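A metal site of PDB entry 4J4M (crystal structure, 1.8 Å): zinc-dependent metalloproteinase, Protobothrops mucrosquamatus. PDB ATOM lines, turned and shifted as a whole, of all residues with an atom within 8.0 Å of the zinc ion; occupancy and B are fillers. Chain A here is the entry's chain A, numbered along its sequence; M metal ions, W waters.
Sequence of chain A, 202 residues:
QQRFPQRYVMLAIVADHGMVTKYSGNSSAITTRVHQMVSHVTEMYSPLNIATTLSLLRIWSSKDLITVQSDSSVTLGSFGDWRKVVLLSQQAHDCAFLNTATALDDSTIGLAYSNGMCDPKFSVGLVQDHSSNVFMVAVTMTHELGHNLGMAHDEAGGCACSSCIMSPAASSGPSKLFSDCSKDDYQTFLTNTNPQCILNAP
O of Met 151 sits at hydrogen-bond distance from ND1 of His 147 (3.1 Å). A ring nitrogen (ND1) of His 143 sits at hydrogen-bond distance from the backbone carbonyl oxygen of Ile 165 (2.8 Å).
Of the 18 residues printed, 3 come within 4 Å of the zinc ion. Along chain A the residues within 4 Å of the zinc ion span positions 143 to 153.
The zinc ion is bound by NE2 of His 147 (2.0 Å), NE2 of His 153 (2.0 Å), NE2 of His 143 (2.1 Å) and water W1 (2.2 Å).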
ATOM      1  N   GLY A 110      37.469   5.612  11.645  1.00  0.00           N
ATOM      2  CA  GLY A 110      37.066   6.764  10.869  1.00  0.00           C
ATOM      3  C   GLY A 110      37.038   8.061  11.659  1.00  0.00           C
ATOM      4  O   GLY A 110      37.129   8.036  12.887  1.00  0.00           O
ATOM      5  N   LEU A 111      36.935   9.179  10.964  1.00  0.00           N
ATOM      6  CA  LEU A 111      36.878  10.487  11.607  1.00  0.00           C
ATOM      7  C   LEU A 111      36.340  11.515  10.608  1.00  0.00           C
ATOM      8  O   LEU A 111      36.560  11.384   9.407  1.00  0.00           O
ATOM      9  CB  LEU A 111      38.280  10.914  12.061  1.00  0.00           C
ATOM     10  CG  LEU A 111      38.361  12.140  12.978  1.00  0.00           C
ATOM     11  CD1 LEU A 111      37.844  11.750  14.355  1.00  0.00           C
ATOM     12  CD2 LEU A 111      39.799  12.650  13.083  1.00  0.00           C
ATOM     13  N   ALA A 112      35.619  12.518  11.114  1.00  0.00           N
ATOM     14  CA  ALA A 112      35.070  13.556  10.260  1.00  0.00           C
ATOM     15  C   ALA A 112      34.791  14.800  11.082  1.00  0.00           C
ATOM     16  O   ALA A 112      34.718  14.739  12.309  1.00  0.00           O
ATOM     17  CB  ALA A 112      33.773  13.065   9.613  1.00  0.00           C
ATOM     18  N   SER A 114      32.291  17.434  12.419  1.00  0.00           N
ATOM     19  CA  SER A 114      30.865  17.598  12.610  1.00  0.00           C
ATOM     20  C   SER A 114      30.411  18.909  11.962  1.00  0.00           C
ATOM     21  O   SER A 114      31.069  19.954  12.126  1.00  0.00           O
ATOM     22  CB  SER A 114      30.513  17.599  14.104  1.00  0.00           C
ATOM     23  OG  SER A 114      30.736  16.318  14.681  1.00  0.00           O
ATOM     24  N   THR A 140      30.875   2.715   7.360  1.00  0.00           N
ATOM     25  CA  THR A 140      31.738   3.649   8.082  1.00  0.00           C
ATOM     26  C   THR A 140      31.798   4.982   7.323  1.00  0.00           C
ATOM     27  O   THR A 140      31.683   6.044   7.927  1.00  0.00           O
ATOM     28  CB  THR A 140      33.174   3.096   8.236  1.00  0.00           C
ATOM     29  OG1 THR A 140      33.130   1.874   9.000  1.00  0.00           O
ATOM     30  CG2 THR A 140      34.073   4.103   8.948  1.00  0.00           C
ATOM     31  N   HIS A 143      28.664   6.746   7.853  1.00  0.00           N
ATOM     32  CA  HIS A 143      28.657   7.224   9.232  1.00  0.00           C
ATOM     33  C   HIS A 143      29.421   8.547   9.326  1.00  0.00           C
ATOM     34  O   HIS A 143      28.934   9.501   9.942  1.00  0.00           O
ATOM     35  CB  HIS A 143      29.320   6.163  10.130  1.00  0.00           C
ATOM     36  CG  HIS A 143      29.443   6.564  11.565  1.00  0.00           C
ATOM     37  ND1 HIS A 143      28.669   5.993  12.565  1.00  0.00           N
ATOM     38  CD2 HIS A 143      30.276   7.417  12.193  1.00  0.00           C
ATOM     39  CE1 HIS A 143      29.038   6.476  13.735  1.00  0.00           C
ATOM     40  NE2 HIS A 143      30.013   7.344  13.542  1.00  0.00           N
ATOM     41  N   GLU A 144      30.605   8.596   8.728  1.00  0.00           N
ATOM     42  CA  GLU A 144      31.421   9.818   8.768  1.00  0.00           C
ATOM     43  C   GLU A 144      30.769  10.932   7.954  1.00  0.00           C
ATOM     44  O   GLU A 144      30.868  12.101   8.314  1.00  0.00           O
ATOM     45  CB  GLU A 144      32.839   9.538   8.252  1.00  0.00           C
ATOM     46  CG  GLU A 144      33.569   8.422   9.015  1.00  0.00           C
ATOM     47  CD  GLU A 144      33.676   8.689  10.513  1.00  0.00           C
ATOM     48  OE1 GLU A 144      33.880   7.719  11.265  1.00  0.00           O
ATOM     49  OE2 GLU A 144      33.564   9.860  10.933  1.00  0.00           O
ATOM     50  N   GLY A 146      27.757  11.246   7.832  1.00  0.00           N
ATOM     51  CA  GLY A 146      26.697  11.605   8.762  1.00  0.00           C
ATOM     52  C   GLY A 146      27.136  12.731   9.684  1.00  0.00           C
ATOM     53  O   GLY A 146      26.382  13.679   9.915  1.00  0.00           O
ATOM     54  N   HIS A 147      28.348  12.624  10.215  1.00  0.00           N
ATOM     55  CA  HIS A 147      28.901  13.657  11.084  1.00  0.00           C
ATOM     56  C   HIS A 147      29.046  14.947  10.278  1.00  0.00           C
ATOM     57  O   HIS A 147      28.717  16.026  10.768  1.00  0.00           O
ATOM     58  CB  HIS A 147      30.265  13.227  11.634  1.00  0.00           C
ATOM     59  CG  HIS A 147      30.194  12.212  12.725  1.00  0.00           C
ATOM     60  ND1 HIS A 147      29.475  12.412  13.893  1.00  0.00           N
ATOM     61  CD2 HIS A 147      30.759  10.988  12.852  1.00  0.00           C
ATOM     62  CE1 HIS A 147      29.599  11.356  14.676  1.00  0.00           C
ATOM     63  NE2 HIS A 147      30.381  10.475  14.070  1.00  0.00           N
ATOM     64  N   MET A 151      25.044  14.984  12.112  1.00  0.00           N
ATOM     65  CA  MET A 151      24.511  13.912  12.943  1.00  0.00           C
ATOM     66  C   MET A 151      25.435  13.538  14.097  1.00  0.00           C
ATOM     67  O   MET A 151      26.650  13.561  13.963  1.00  0.00           O
ATOM     68  CB  MET A 151      24.255  12.661  12.107  1.00  0.00           C
ATOM     69  CG  MET A 151      23.254  12.862  11.009  1.00  0.00           C
ATOM     70  SD  MET A 151      23.155  11.382   9.985  1.00  0.00           S
ATOM     71  CE  MET A 151      22.219  12.030   8.597  1.00  0.00           C
ATOM     72  N   ALA A 152      24.835  13.199  15.234  1.00  0.00           N
ATOM     73  CA  ALA A 152      25.581  12.783  16.413  1.00  0.00           C
ATOM     74  C   ALA A 152      25.338  11.283  16.571  1.00  0.00           C
ATOM     75  O   ALA A 152      24.544  10.695  15.849  1.00  0.00           O
ATOM     76  CB  ALA A 152      25.104  13.545  17.652  1.00  0.00           C
ATOM     77  N   HIS A 153      26.025  10.668  17.534  1.00  0.00           N
ATOM     78  CA  HIS A 153      25.884   9.231  17.773  1.00  0.00           C
ATOM     79  C   HIS A 153      24.550   8.826  18.378  1.00  0.00           C
ATOM     80  O   HIS A 153      23.882   9.606  19.064  1.00  0.00           O
ATOM     81  CB  HIS A 153      27.010   8.750  18.689  1.00  0.00           C
ATOM     82  CG  HIS A 153      28.350   8.688  18.020  1.00  0.00           C
ATOM     83  ND1 HIS A 153      29.528   8.590  18.713  1.00  0.00           N
ATOM     84  CD2 HIS A 153      28.685   8.681  16.707  1.00  0.00           C
ATOM     85  CE1 HIS A 153      30.540   8.531  17.869  1.00  0.00           C
ATOM     86  NE2 HIS A 153      30.055   8.583  16.645  1.00  0.00           N
ATOM     87  N   ASP A 154      24.150   7.583  18.110  1.00  0.00           N
ATOM     88  CA  ASP A 154      22.908   7.064  18.664  1.00  0.00           C
ATOM     89  C   ASP A 154      23.233   6.540  20.054  1.00  0.00           C
ATOM     90  O   ASP A 154      23.540   5.362  20.231  1.00  0.00           O
ATOM     91  CB  ASP A 154      22.367   5.916  17.805  1.00  0.00           C
ATOM     92  CG  ASP A 154      21.787   6.408  16.492  1.00  0.00           C
ATOM     93  OD1 ASP A 154      21.163   7.482  16.501  1.00  0.00           O
ATOM     94  OD2 ASP A 154      21.953   5.720  15.467  1.00  0.00           O
ATOM     95  N   ILE A 165      23.142   3.285  11.412  1.00  0.00           N
ATOM     96  CA  ILE A 165      24.367   3.847  10.853  1.00  0.00           C
ATOM     97  C   ILE A 165      25.186   4.676  11.836  1.00  0.00           C
ATOM     98  O   ILE A 165      26.406   4.486  11.938  1.00  0.00           O
ATOM     99  CB  ILE A 165      24.058   4.707   9.608  1.00  0.00           C
ATOM    100  CG1 ILE A 165      23.445   3.826   8.513  1.00  0.00           C
ATOM    101  CG2 ILE A 165      25.333   5.382   9.091  1.00  0.00           C
ATOM    102  CD1 ILE A 165      22.945   4.591   7.300  1.00  0.00           C
ATOM    103  N   MET A 166      24.539   5.580  12.561  1.00  0.00           N
ATOM    104  CA  MET A 166      25.245   6.451  13.503  1.00  0.00           C
ATOM    105  C   MET A 166      25.517   5.840  14.877  1.00  0.00           C
ATOM    106  O   MET A 166      25.725   6.561  15.854  1.00  0.00           O
ATOM    107  CB  MET A 166      24.492   7.773  13.657  1.00  0.00           C
ATOM    108  CG  MET A 166      24.429   8.585  12.378  1.00  0.00           C
ATOM    109  SD  MET A 166      26.043   8.721  11.566  1.00  0.00           S
ATOM    110  CE  MET A 166      26.927   9.755  12.735  1.00  0.00           C
ATOM    111  N   SER A 167      25.521   4.520  14.936  1.00  0.00           N
ATOM    112  CA  SER A 167      25.818   3.843  16.186  1.00  0.00           C
ATOM    113  C   SER A 167      27.274   4.143  16.509  1.00  0.00           C
ATOM    114  O   SER A 167      28.107   4.192  15.607  1.00  0.00           O
ATOM    115  CB  SER A 167      25.622   2.338  16.020  1.00  0.00           C
ATOM    116  OG  SER A 167      25.874   1.670  17.234  1.00  0.00           O
ATOM    117  N   PRO A 168      27.602   4.347  17.791  1.00  0.00           N
ATOM    118  CA  PRO A 168      28.992   4.643  18.144  1.00  0.00           C
ATOM    119  C   PRO A 168      29.968   3.499  17.845  1.00  0.00           C
ATOM    120  O   PRO A 168      31.131   3.745  17.532  1.00  0.00           O
ATOM    121  CB  PRO A 168      28.903   4.988  19.627  1.00  0.00           C
ATOM    122  CG  PRO A 168      27.709   4.208  20.104  1.00  0.00           C
ATOM    123  CD  PRO A 168      26.722   4.413  18.978  1.00  0.00           C
ATOM    124  N   ALA A 169      29.504   2.261  17.950  1.00  0.00           N
ATOM    125  CA  ALA A 169      30.364   1.103  17.682  1.00  0.00           C
ATOM    126  C   ALA A 169      29.889   0.350  16.449  1.00  0.00           C
ATOM    127  O   ALA A 169      28.684   0.232  16.204  1.00  0.00           O
ATOM    128  CB  ALA A 169      30.389   0.173  18.899  1.00  0.00           C
HETATM  129 ZN    ZN M   1      31.034   8.703  14.851  1.00  0.00          ZN
HETATM  130  O   HOH W   1      33.174   8.494  14.268  1.00  0.00           O
